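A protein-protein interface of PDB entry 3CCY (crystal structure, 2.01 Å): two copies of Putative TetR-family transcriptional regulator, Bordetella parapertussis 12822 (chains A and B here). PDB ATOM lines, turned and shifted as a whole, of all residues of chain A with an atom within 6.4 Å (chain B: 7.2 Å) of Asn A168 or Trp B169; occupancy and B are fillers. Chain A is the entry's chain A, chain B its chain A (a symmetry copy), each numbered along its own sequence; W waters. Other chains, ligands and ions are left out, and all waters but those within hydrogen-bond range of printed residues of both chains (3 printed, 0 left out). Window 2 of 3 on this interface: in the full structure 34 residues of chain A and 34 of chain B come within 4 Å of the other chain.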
ATOM      1  N   PHE A  98      17.003  24.943  -9.614  1.00  0.00           N
ATOM      2  CA  PHE A  98      18.272  24.730  -8.897  1.00  0.00           C
ATOM      3  C   PHE A  98      18.430  23.277  -8.489  1.00  0.00           C
ATOM      4  O   PHE A  98      19.518  22.689  -8.631  1.00  0.00           O
ATOM      5  CB  PHE A  98      18.459  25.716  -7.711  1.00  0.00           C
ATOM      6  CG  PHE A  98      18.572  27.175  -8.134  1.00  0.00           C
ATOM      7  CD1 PHE A  98      18.641  27.527  -9.470  1.00  0.00           C
ATOM      8  CD2 PHE A  98      18.644  28.186  -7.204  1.00  0.00           C
ATOM      9  CE1 PHE A  98      18.751  28.860  -9.853  1.00  0.00           C
ATOM     10  CE2 PHE A  98      18.761  29.535  -7.593  1.00  0.00           C
ATOM     11  CZ  PHE A  98      18.821  29.862  -8.901  1.00  0.00           C
ATOM     12  N   HIS A 109      28.037  21.165  -9.707  1.00  0.00           N
ATOM     13  CA  HIS A 109      27.328  21.932  -8.659  1.00  0.00           C
ATOM     14  C   HIS A 109      28.152  21.990  -7.361  1.00  0.00           C
ATOM     15  O   HIS A 109      28.485  23.064  -6.852  1.00  0.00           O
ATOM     16  CB  HIS A 109      25.975  21.257  -8.410  1.00  0.00           C
ATOM     17  CG  HIS A 109      24.935  22.132  -7.778  1.00  0.00           C
ATOM     18  ND1 HIS A 109      24.751  22.202  -6.409  1.00  0.00           N
ATOM     19  CD2 HIS A 109      23.987  22.932  -8.331  1.00  0.00           C
ATOM     20  CE1 HIS A 109      23.740  23.020  -6.150  1.00  0.00           C
ATOM     21  NE2 HIS A 109      23.253  23.469  -7.299  1.00  0.00           N
ATOM     22  N   MET A 112      31.144  24.218  -7.800  1.00  0.00           N
ATOM     23  CA  MET A 112      30.724  25.635  -7.694  1.00  0.00           C
ATOM     24  C   MET A 112      30.713  26.023  -6.207  1.00  0.00           C
ATOM     25  O   MET A 112      31.461  26.907  -5.763  1.00  0.00           O
ATOM     26  CB  MET A 112      29.322  25.876  -8.342  1.00  0.00           C
ATOM     27  CG  MET A 112      28.835  27.383  -8.447  1.00  0.00           C
ATOM     28  SD  MET A 112      27.075  27.846  -9.315  1.00  0.00           S
ATOM     29  CE  MET A 112      25.933  26.707  -8.214  1.00  0.00           C
ATOM     30  N   LEU A 113      29.862  25.327  -5.447  1.00  0.00           N
ATOM     31  CA  LEU A 113      29.636  25.568  -4.010  1.00  0.00           C
ATOM     32  C   LEU A 113      30.854  25.371  -3.120  1.00  0.00           C
ATOM     33  O   LEU A 113      30.795  25.695  -1.942  1.00  0.00           O
ATOM     34  CB  LEU A 113      28.476  24.693  -3.496  1.00  0.00           C
ATOM     35  CG  LEU A 113      27.130  24.886  -4.217  1.00  0.00           C
ATOM     36  CD1 LEU A 113      26.033  23.976  -3.690  1.00  0.00           C
ATOM     37  CD2 LEU A 113      26.662  26.369  -4.189  1.00  0.00           C
ATOM     38  N   THR A 114      31.960  24.872  -3.666  1.00  0.00           N
ATOM     39  CA  THR A 114      33.054  24.354  -2.827  1.00  0.00           C
ATOM     40  C   THR A 114      34.476  24.777  -3.215  1.00  0.00           C
ATOM     41  O   THR A 114      35.361  24.820  -2.356  1.00  0.00           O
ATOM     42  CB  THR A 114      32.964  22.788  -2.738  1.00  0.00           C
ATOM     43  OG1 THR A 114      32.097  22.414  -1.657  1.00  0.00           O
ATOM     44  CG2 THR A 114      34.339  22.118  -2.557  1.00  0.00           C
ATOM     45  N   MET A 161      19.865  34.826   1.902  1.00  0.00           N
ATOM     46  CA  MET A 161      20.978  33.935   2.183  1.00  0.00           C
ATOM     47  C   MET A 161      20.532  32.766   3.098  1.00  0.00           C
ATOM     48  O   MET A 161      21.081  31.689   3.025  1.00  0.00           O
ATOM     49  CB  MET A 161      22.164  34.725   2.799  1.00  0.00           C
ATOM     50  CG  MET A 161      22.753  35.792   1.889  1.00  0.00           C
ATOM     51  SD  MET A 161      23.049  35.136   0.079  1.00  0.00           S
ATOM     52  CE  MET A 161      24.608  34.090   0.526  1.00  0.00           C
ATOM     53  N   LEU A 162      19.506  32.980   3.931  1.00  0.00           N
ATOM     54  CA  LEU A 162      18.978  31.872   4.736  1.00  0.00           C
ATOM     55  C   LEU A 162      18.289  30.865   3.827  1.00  0.00           C
ATOM     56  O   LEU A 162      18.494  29.661   3.954  1.00  0.00           O
ATOM     57  CB  LEU A 162      18.020  32.369   5.800  1.00  0.00           C
ATOM     58  CG  LEU A 162      18.724  33.102   6.960  1.00  0.00           C
ATOM     59  CD1 LEU A 162      17.727  33.881   7.829  1.00  0.00           C
ATOM     60  CD2 LEU A 162      19.635  32.133   7.846  1.00  0.00           C
ATOM     61  N   PHE A 163      17.524  31.390   2.872  1.00  0.00           N
ATOM     62  CA  PHE A 163      16.994  30.563   1.831  1.00  0.00           C
ATOM     63  C   PHE A 163      18.072  29.767   1.061  1.00  0.00           C
ATOM     64  O   PHE A 163      17.910  28.562   0.903  1.00  0.00           O
ATOM     65  CB  PHE A 163      16.147  31.354   0.851  1.00  0.00           C
ATOM     66  CG  PHE A 163      15.810  30.542  -0.352  1.00  0.00           C
ATOM     67  CD1 PHE A 163      14.806  29.576  -0.273  1.00  0.00           C
ATOM     68  CD2 PHE A 163      16.584  30.629  -1.502  1.00  0.00           C
ATOM     69  CE1 PHE A 163      14.535  28.747  -1.359  1.00  0.00           C
ATOM     70  CE2 PHE A 163      16.318  29.783  -2.576  1.00  0.00           C
ATOM     71  CZ  PHE A 163      15.295  28.861  -2.485  1.00  0.00           C
ATOM     72  N   PHE A 164      19.083  30.452   0.506  1.00  0.00           N
ATOM     73  CA  PHE A 164      20.200  29.750  -0.175  1.00  0.00           C
ATOM     74  C   PHE A 164      20.841  28.607   0.607  1.00  0.00           C
ATOM     75  O   PHE A 164      21.163  27.564   0.055  1.00  0.00           O
ATOM     76  CB  PHE A 164      21.267  30.713  -0.693  1.00  0.00           C
ATOM     77  CG  PHE A 164      20.951  31.219  -2.080  1.00  0.00           C
ATOM     78  CD1 PHE A 164      20.948  30.343  -3.166  1.00  0.00           C
ATOM     79  CD2 PHE A 164      20.580  32.544  -2.288  1.00  0.00           C
ATOM     80  CE1 PHE A 164      20.625  30.788  -4.467  1.00  0.00           C
ATOM     81  CE2 PHE A 164      20.243  32.992  -3.586  1.00  0.00           C
ATOM     82  CZ  PHE A 164      20.273  32.117  -4.659  1.00  0.00           C
ATOM     83  N   GLY A 165      21.057  28.833   1.881  1.00  0.00           N
ATOM     84  CA  GLY A 165      21.499  27.783   2.812  1.00  0.00           C
ATOM     85  C   GLY A 165      20.669  26.518   2.751  1.00  0.00           C
ATOM     86  O   GLY A 165      21.245  25.430   2.694  1.00  0.00           O
ATOM     87  N   MET A 166      19.336  26.637   2.813  1.00  0.00           N
ATOM     88  CA  MET A 166      18.477  25.441   2.694  1.00  0.00           C
ATOM     89  C   MET A 166      18.772  24.626   1.475  1.00  0.00           C
ATOM     90  O   MET A 166      18.851  23.397   1.560  1.00  0.00           O
ATOM     91  CB  MET A 166      16.994  25.794   2.548  1.00  0.00           C
ATOM     92  CG  MET A 166      16.409  26.491   3.691  1.00  0.00           C
ATOM     93  SD  MET A 166      14.442  26.596   3.335  1.00  0.00           S
ATOM     94  CE  MET A 166      14.212  28.346   3.678  1.00  0.00           C
ATOM     95  N   ILE A 167      18.822  25.299   0.316  1.00  0.00           N
ATOM     96  CA  ILE A 167      19.059  24.572  -0.941  1.00  0.00           C
ATOM     97  C   ILE A 167      20.516  24.248  -1.242  1.00  0.00           C
ATOM     98  O   ILE A 167      20.777  23.216  -1.816  1.00  0.00           O
ATOM     99  CB  ILE A 167      18.410  25.264  -2.202  1.00  0.00           C
ATOM    100  CG1 ILE A 167      18.872  26.708  -2.416  1.00  0.00           C
ATOM    101  CG2 ILE A 167      16.892  25.170  -2.166  1.00  0.00           C
ATOM    102  CD1 ILE A 167      18.556  27.110  -3.886  1.00  0.00           C
ATOM    103  N   ASN A 168      21.461  25.122  -0.893  1.00  0.00           N
ATOM    104  CA  ASN A 168      22.893  24.872  -1.166  1.00  0.00           C
ATOM    105  C   ASN A 168      23.477  23.791  -0.263  1.00  0.00           C
ATOM    106  O   ASN A 168      24.443  23.112  -0.661  1.00  0.00           O
ATOM    107  CB  ASN A 168      23.755  26.151  -1.053  1.00  0.00           C
ATOM    108  CG  ASN A 168      23.498  27.133  -2.186  1.00  0.00           C
ATOM    109  OD1 ASN A 168      22.745  26.834  -3.097  1.00  0.00           O
ATOM    110  ND2 ASN A 168      24.116  28.312  -2.132  1.00  0.00           N
ATOM    111  N   TRP A 169      22.933  23.619   0.948  1.00  0.00           N
ATOM    112  CA  TRP A 169      23.410  22.572   1.872  1.00  0.00           C
ATOM    113  C   TRP A 169      23.029  21.156   1.459  1.00  0.00           C
ATOM    114  O   TRP A 169      23.568  20.193   2.005  1.00  0.00           O
ATOM    115  CB  TRP A 169      22.886  22.825   3.312  1.00  0.00           C
ATOM    116  CG  TRP A 169      23.572  22.063   4.406  1.00  0.00           C
ATOM    117  CD1 TRP A 169      23.012  21.137   5.264  1.00  0.00           C
ATOM    118  CD2 TRP A 169      24.939  22.140   4.736  1.00  0.00           C
ATOM    119  NE1 TRP A 169      23.968  20.661   6.118  1.00  0.00           N
ATOM    120  CE2 TRP A 169      25.161  21.266   5.815  1.00  0.00           C
ATOM    121  CE3 TRP A 169      26.011  22.881   4.226  1.00  0.00           C
ATOM    122  CZ2 TRP A 169      26.414  21.105   6.401  1.00  0.00           C
ATOM    123  CZ3 TRP A 169      27.258  22.729   4.829  1.00  0.00           C
ATOM    124  CH2 TRP A 169      27.447  21.842   5.884  1.00  0.00           C
ATOM    125  N   THR A 170      22.124  21.035   0.493  1.00  0.00           N
ATOM    126  CA  THR A 170      21.608  19.730   0.042  1.00  0.00           C
ATOM    127  C   THR A 170      22.685  18.752  -0.413  1.00  0.00           C
ATOM    128  O   THR A 170      22.563  17.554  -0.228  1.00  0.00           O
ATOM    129  CB  THR A 170      20.514  19.866  -1.058  1.00  0.00           C
ATOM    130  OG1 THR A 170      20.976  20.698  -2.128  1.00  0.00           O
ATOM    131  CG2 THR A 170      19.211  20.498  -0.425  1.00  0.00           C
ATOM    132  N   TYR A 171      23.749  19.269  -0.989  1.00  0.00           N
ATOM    133  CA  TYR A 171      24.824  18.391  -1.451  1.00  0.00           C
ATOM    134  C   TYR A 171      25.375  17.531  -0.314  1.00  0.00           C
ATOM    135  O   TYR A 171      25.902  16.440  -0.556  1.00  0.00           O
ATOM    136  CB  TYR A 171      25.922  19.184  -2.174  1.00  0.00           C
ATOM    137  CG  TYR A 171      26.941  19.861  -1.289  1.00  0.00           C
ATOM    138  CD1 TYR A 171      28.147  19.229  -0.967  1.00  0.00           C
ATOM    139  CD2 TYR A 171      26.730  21.141  -0.808  1.00  0.00           C
ATOM    140  CE1 TYR A 171      29.079  19.846  -0.153  1.00  0.00           C
ATOM    141  CE2 TYR A 171      27.671  21.762   0.025  1.00  0.00           C
ATOM    142  CZ  TYR A 171      28.821  21.120   0.323  1.00  0.00           C
ATOM    143  OH  TYR A 171      29.719  21.759   1.135  1.00  0.00           O
ATOM    144  N   THR A 172      25.249  17.999   0.923  1.00  0.00           N
ATOM    145  CA  THR A 172      25.835  17.246   2.046  1.00  0.00           C
ATOM    146  C   THR A 172      24.971  16.059   2.493  1.00  0.00           C
ATOM    147  O   THR A 172      25.453  15.203   3.241  1.00  0.00           O
ATOM    148  CB  THR A 172      26.096  18.126   3.308  1.00  0.00           C
ATOM    149  OG1 THR A 172      24.839  18.591   3.866  1.00  0.00           O
ATOM    150  CG2 THR A 172      26.971  19.326   2.949  1.00  0.00           C
ATOM    151  N   TYR B 102      29.101  29.851  16.589  1.00  0.00           N
ATOM    152  CA  TYR B 102      29.686  30.561  15.422  1.00  0.00           C
ATOM    153  C   TYR B 102      30.356  31.930  15.740  1.00  0.00           C
ATOM    154  O   TYR B 102      31.510  32.202  15.358  1.00  0.00           O
ATOM    155  CB  TYR B 102      28.600  30.738  14.370  1.00  0.00           C
ATOM    156  CG  TYR B 102      29.083  31.417  13.113  1.00  0.00           C
ATOM    157  CD1 TYR B 102      29.766  30.689  12.117  1.00  0.00           C
ATOM    158  CD2 TYR B 102      28.844  32.781  12.908  1.00  0.00           C
ATOM    159  CE1 TYR B 102      30.212  31.302  10.956  1.00  0.00           C
ATOM    160  CE2 TYR B 102      29.278  33.399  11.744  1.00  0.00           C
ATOM    161  CZ  TYR B 102      29.966  32.658  10.775  1.00  0.00           C
ATOM    162  OH  TYR B 102      30.399  33.280   9.650  1.00  0.00           O
ATOM    163  N   HIS B 109      34.204  25.771  14.150  1.00  0.00           N
ATOM    164  CA  HIS B 109      32.885  25.528  13.525  1.00  0.00           C
ATOM    165  C   HIS B 109      33.031  25.219  12.025  1.00  0.00           C
ATOM    166  O   HIS B 109      32.606  24.168  11.534  1.00  0.00           O
ATOM    167  CB  HIS B 109      32.021  26.775  13.739  1.00  0.00           C
ATOM    168  CG  HIS B 109      30.543  26.549  13.632  1.00  0.00           C
ATOM    169  ND1 HIS B 109      29.848  26.706  12.446  1.00  0.00           N
ATOM    170  CD2 HIS B 109      29.620  26.232  14.576  1.00  0.00           C
ATOM    171  CE1 HIS B 109      28.561  26.482  12.667  1.00  0.00           C
ATOM    172  NE2 HIS B 109      28.393  26.202  13.953  1.00  0.00           N
ATOM    173  N   LEU B 113      32.130  21.673   9.942  1.00  0.00           N
ATOM    174  CA  LEU B 113      31.296  21.705   8.727  1.00  0.00           C
ATOM    175  C   LEU B 113      32.030  21.399   7.429  1.00  0.00           C
ATOM    176  O   LEU B 113      31.389  21.255   6.397  1.00  0.00           O
ATOM    177  CB  LEU B 113      30.580  23.064   8.603  1.00  0.00           C
ATOM    178  CG  LEU B 113      29.683  23.451   9.792  1.00  0.00           C
ATOM    179  CD1 LEU B 113      29.028  24.813   9.632  1.00  0.00           C
ATOM    180  CD2 LEU B 113      28.607  22.366  10.086  1.00  0.00           C
ATOM    181  N   PHE B 163      16.294  22.883   7.501  1.00  0.00           N
ATOM    182  CA  PHE B 163      16.645  23.757   8.580  1.00  0.00           C
ATOM    183  C   PHE B 163      18.169  23.880   8.807  1.00  0.00           C
ATOM    184  O   PHE B 163      18.659  25.001   8.897  1.00  0.00           O
ATOM    185  CB  PHE B 163      15.967  23.359   9.878  1.00  0.00           C
ATOM    186  CG  PHE B 163      16.526  24.113  11.035  1.00  0.00           C
ATOM    187  CD1 PHE B 163      16.141  25.439  11.246  1.00  0.00           C
ATOM    188  CD2 PHE B 163      17.539  23.566  11.812  1.00  0.00           C
ATOM    189  CE1 PHE B 163      16.718  26.188  12.268  1.00  0.00           C
ATOM    190  CE2 PHE B 163      18.123  24.329  12.820  1.00  0.00           C
ATOM    191  CZ  PHE B 163      17.698  25.625  13.031  1.00  0.00           C
ATOM    192  N   PHE B 164      18.870  22.753   9.006  1.00  0.00           N
ATOM    193  CA  PHE B 164      20.347  22.786   9.145  1.00  0.00           C
ATOM    194  C   PHE B 164      21.098  23.569   8.073  1.00  0.00           C
ATOM    195  O   PHE B 164      22.049  24.284   8.359  1.00  0.00           O
ATOM    196  CB  PHE B 164      20.949  21.392   9.315  1.00  0.00           C
ATOM    197  CG  PHE B 164      20.982  20.959  10.761  1.00  0.00           C
ATOM    198  CD1 PHE B 164      21.795  21.626  11.677  1.00  0.00           C
ATOM    199  CD2 PHE B 164      20.146  19.946  11.221  1.00  0.00           C
ATOM    200  CE1 PHE B 164      21.818  21.258  13.041  1.00  0.00           C
ATOM    201  CE2 PHE B 164      20.156  19.582  12.587  1.00  0.00           C
ATOM    202  CZ  PHE B 164      20.990  20.234  13.479  1.00  0.00           C
ATOM    203  N   GLY B 165      20.687  23.394   6.839  1.00  0.00           N
ATOM    204  CA  GLY B 165      21.180  24.203   5.713  1.00  0.00           C
ATOM    205  C   GLY B 165      21.126  25.696   5.958  1.00  0.00           C
ATOM    206  O   GLY B 165      22.116  26.380   5.689  1.00  0.00           O
ATOM    207  N   MET B 166      19.979  26.217   6.414  1.00  0.00           N
ATOM    208  CA  MET B 166      19.891  27.657   6.730  1.00  0.00           C
ATOM    209  C   MET B 166      20.965  28.119   7.664  1.00  0.00           C
ATOM    210  O   MET B 166      21.568  29.172   7.436  1.00  0.00           O
ATOM    211  CB  MET B 166      18.594  28.022   7.457  1.00  0.00           C
ATOM    212  CG  MET B 166      17.371  27.792   6.691  1.00  0.00           C
ATOM    213  SD  MET B 166      15.879  28.580   7.769  1.00  0.00           S
ATOM    214  CE  MET B 166      14.752  27.180   7.709  1.00  0.00           C
ATOM    215  N   ILE B 167      21.128  27.391   8.779  1.00  0.00           N
ATOM    216  CA  ILE B 167      22.128  27.799   9.777  1.00  0.00           C
ATOM    217  C   ILE B 167      23.560  27.377   9.475  1.00  0.00           C
ATOM    218  O   ILE B 167      24.465  28.108   9.806  1.00  0.00           O
ATOM    219  CB  ILE B 167      21.760  27.369  11.250  1.00  0.00           C
ATOM    220  CG1 ILE B 167      21.539  25.863  11.414  1.00  0.00           C
ATOM    221  CG2 ILE B 167      20.575  28.161  11.779  1.00  0.00           C
ATOM    222  CD1 ILE B 167      21.652  25.514  12.927  1.00  0.00           C
ATOM    223  N   ASN B 168      23.779  26.202   8.883  1.00  0.00           N
ATOM    224  CA  ASN B 168      25.147  25.729   8.572  1.00  0.00           C
ATOM    225  C   ASN B 168      25.778  26.498   7.416  1.00  0.00           C
ATOM    226  O   ASN B 168      27.017  26.607   7.353  1.00  0.00           O
ATOM    227  CB  ASN B 168      25.200  24.214   8.269  1.00  0.00           C
ATOM    228  CG  ASN B 168      24.963  23.360   9.505  1.00  0.00           C
ATOM    229  OD1 ASN B 168      24.841  23.885  10.598  1.00  0.00           O
ATOM    230  ND2 ASN B 168      24.890  22.040   9.337  1.00  0.00           N
ATOM    231  N   TRP B 169      24.966  27.019   6.488  1.00  0.00           N
ATOM    232  CA  TRP B 169      25.488  27.808   5.355  1.00  0.00           C
ATOM    233  C   TRP B 169      25.997  29.191   5.742  1.00  0.00           C
ATOM    234  O   TRP B 169      26.672  29.841   4.942  1.00  0.00           O
ATOM    235  CB  TRP B 169      24.410  27.968   4.250  1.00  0.00           C
ATOM    236  CG  TRP B 169      24.902  28.426   2.910  1.00  0.00           C
ATOM    237  CD1 TRP B 169      24.562  29.585   2.240  1.00  0.00           C
ATOM    238  CD2 TRP B 169      25.838  27.755   2.099  1.00  0.00           C
ATOM    239  NE1 TRP B 169      25.228  29.642   1.047  1.00  0.00           N
ATOM    240  CE2 TRP B 169      26.017  28.526   0.937  1.00  0.00           C
ATOM    241  CE3 TRP B 169      26.544  26.555   2.238  1.00  0.00           C
ATOM    242  CZ2 TRP B 169      26.876  28.142  -0.090  1.00  0.00           C
ATOM    243  CZ3 TRP B 169      27.388  26.167   1.199  1.00  0.00           C
ATOM    244  CH2 TRP B 169      27.555  26.962   0.070  1.00  0.00           C
ATOM    245  N   THR B 170      25.691  29.625   6.960  1.00  0.00           N
ATOM    246  CA  THR B 170      26.054  30.969   7.443  1.00  0.00           C
ATOM    247  C   THR B 170      27.543  31.285   7.363  1.00  0.00           C
ATOM    248  O   THR B 170      27.933  32.414   7.122  1.00  0.00           O
ATOM    249  CB  THR B 170      25.527  31.252   8.882  1.00  0.00           C
ATOM    250  OG1 THR B 170      25.913  30.201   9.775  1.00  0.00           O
ATOM    251  CG2 THR B 170      23.951  31.363   8.849  1.00  0.00           C
ATOM    252  N   TYR B 171      28.372  30.279   7.543  1.00  0.00           N
ATOM    253  CA  TYR B 171      29.815  30.506   7.480  1.00  0.00           C
ATOM    254  C   TYR B 171      30.230  31.118   6.142  1.00  0.00           C
ATOM    255  O   TYR B 171      31.250  31.809   6.060  1.00  0.00           O
ATOM    256  CB  TYR B 171      30.599  29.229   7.811  1.00  0.00           C
ATOM    257  CG  TYR B 171      30.768  28.244   6.678  1.00  0.00           C
ATOM    258  CD1 TYR B 171      31.908  28.270   5.867  1.00  0.00           C
ATOM    259  CD2 TYR B 171      29.823  27.263   6.438  1.00  0.00           C
ATOM    260  CE1 TYR B 171      32.061  27.373   4.826  1.00  0.00           C
ATOM    261  CE2 TYR B 171      29.975  26.360   5.377  1.00  0.00           C
ATOM    262  CZ  TYR B 171      31.083  26.419   4.608  1.00  0.00           C
ATOM    263  OH  TYR B 171      31.200  25.518   3.584  1.00  0.00           O
ATOM    264  N   THR B 172      29.446  30.884   5.094  1.00  0.00           N
ATOM    265  CA  THR B 172      29.843  31.384   3.766  1.00  0.00           C
ATOM    266  C   THR B 172      29.535  32.873   3.564  1.00  0.00           C
ATOM    267  O   THR B 172      30.039  33.475   2.611  1.00  0.00           O
ATOM    268  CB  THR B 172      29.170  30.610   2.591  1.00  0.00           C
ATOM    269  OG1 THR B 172      27.736  30.840   2.594  1.00  0.00           O
ATOM    270  CG2 THR B 172      29.447  29.113   2.709  1.00  0.00           C
ATOM    271  N   TRP B 173      28.677  33.452   4.397  1.00  0.00           N
ATOM    272  CA  TRP B 173      28.165  34.811   4.095  1.00  0.00           C
ATOM    273  C   TRP B 173      28.029  35.718   5.322  1.00  0.00           C
ATOM    274  O   TRP B 173      28.125  36.959   5.216  1.00  0.00           O
ATOM    275  CB  TRP B 173      26.802  34.721   3.386  1.00  0.00           C
ATOM    276  CG  TRP B 173      25.636  34.120   4.215  1.00  0.00           C
ATOM    277  CD1 TRP B 173      25.213  32.796   4.243  1.00  0.00           C
ATOM    278  CD2 TRP B 173      24.740  34.839   5.069  1.00  0.00           C
ATOM    279  NE1 TRP B 173      24.121  32.663   5.090  1.00  0.00           N
ATOM    280  CE2 TRP B 173      23.802  33.903   5.590  1.00  0.00           C
ATOM    281  CE3 TRP B 173      24.633  36.202   5.450  1.00  0.00           C
ATOM    282  CZ2 TRP B 173      22.801  34.275   6.475  1.00  0.00           C
ATOM    283  CZ3 TRP B 173      23.627  36.564   6.335  1.00  0.00           C
ATOM    284  CH2 TRP B 173      22.718  35.597   6.824  1.00  0.00           C
ATOM    285  N   TYR B 174      27.771  35.107   6.471  1.00  0.00           N
ATOM    286  CA  TYR B 174      27.379  35.873   7.674  1.00  0.00           C
ATOM    287  C   TYR B 174      28.556  36.314   8.519  1.00  0.00           C
ATOM    288  O   TYR B 174      29.447  35.519   8.827  1.00  0.00           O
ATOM    289  CB  TYR B 174      26.397  35.069   8.525  1.00  0.00           C
ATOM    290  CG  TYR B 174      26.079  35.719   9.843  1.00  0.00           C
ATOM    291  CD1 TYR B 174      25.333  36.889   9.891  1.00  0.00           C
ATOM    292  CD2 TYR B 174      26.553  35.160  11.052  1.00  0.00           C
ATOM    293  CE1 TYR B 174      25.031  37.521  11.112  1.00  0.00           C
ATOM    294  CE2 TYR B 174      26.296  35.782  12.275  1.00  0.00           C
ATOM    295  CZ  TYR B 174      25.521  36.957  12.293  1.00  0.00           C
ATOM    296  OH  TYR B 174      25.258  37.570  13.485  1.00  0.00           O
HETATM  297  O   HOH W   1      24.159  18.925   8.424  1.00  0.00           O
HETATM  298  O   HOH W   2      22.321  30.549   5.223  1.00  0.00           O
HETATM  299  O   HOH W   3      25.322  31.304  -1.319  1.00  0.00           O
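Water W2 lies within hydrogen-bond range of the backbone carbonyl oxygen (O) of Met B166, the backbone carbonyl oxygen (O) of Met A161 and the indole nitrogen (NE1) of Trp B173.
Water W1 bridges the indole nitrogen of Trp A169 (2.9 Å) and the side-chain amide nitrogen of Asn B168 (3.3 Å).
Water W3 bridges the indole nitrogen (NE1) of Trp B169 and the side-chain amide nitrogen (ND2) of Asn A168.
Asn A168 touches just one residue of chain B: Trp B169 (3.4 Å).
Printed residues of chain A within 4 Å of Trp B169: Gly A165 and Asn A168.
Printed residues of chain B within 4 Å of Gly A165: Gly B165 (3.3 Å), Met B166 (3.7 Å) and Trp B169 (3.3 Å).
Of the printed residues of chain B, Met A166 touches Gly B165 (3.7 Å) and Met B166 (3.4 Å).
Of the printed residues of chain B, Trp A169 touches Gly B165 (3.3 Å) and Asn B168 (3.4 Å).
Printed residues of chain B within 4 Å of Leu A162: Met B166.
Thr A114 touches none of the printed residues of chain B.
Met A112 touches none of the printed residues of chain B.
The nearest residue of chain B that does not touch Asn A168 is Gly B165 (6.4 Å).
The nearest printed residue of chain A that does not touch Trp B169 is Leu A113 (4.02 Å).
Met A161 touches Trp B173 (CB to CE2, 3.3 Å).
Leu A162 touches Met B166 (O to CG, 3.5 Å).
N of Met B166 touches C of Gly A165 (3.7 Å).
CA of Gly A165 touches CB of Trp B169 (3.3 Å).
Gly B165 touches Met A166.
Met A166 touches Met B166 (CG to CG, 3.4 Å).
ND2 of Asn A168 touches CZ2 of Trp B169, at 3.4 Å.
Trp A169 touches Gly B165 (CB to CA, 3.3 Å).
Trp A169 touches Asn B168.
Gly B165 touches its own counterpart, Gly A165.
Gly A165 touches Trp B169, and with the chains exchanged Trp A169 touches Gly B165.
Met B166 touches its own counterpart, Met A166.
Asn A168 touches Trp B169, and with the chains exchanged Trp A169 touches Asn B168.
12 positions are printed for both chains.
Of the 10 pairs that touch across the chains among the printed residues, 8 have their exchanged pair printed and touching as well.
The backbone carbonyl oxygen (O) of Gly B165 sits close to the backbone carbonyl oxygen (O) of Gly A165 (3.3 Å).
Of the 17 printed residues of chain A, 6 touch a printed residue of chain B.
Of the 15 printed residues of chain B, 5 touch a printed residue of chain A.
Along chain B the printed residues that touch a printed residue of chain A span positions 165 to 173.
Among the printed residues, no Asp or Glu carboxylate lies within 4 Å of a Lys or Arg side-chain nitrogen of the other chain.
O of Trp A169 is in hydrogen-bond range of OG1 of Thr A172 (2.8 Å).
The backbone carbonyl oxygen of Trp B169 sits at hydrogen-bond distance from the side-chain hydroxyl of Thr B172.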
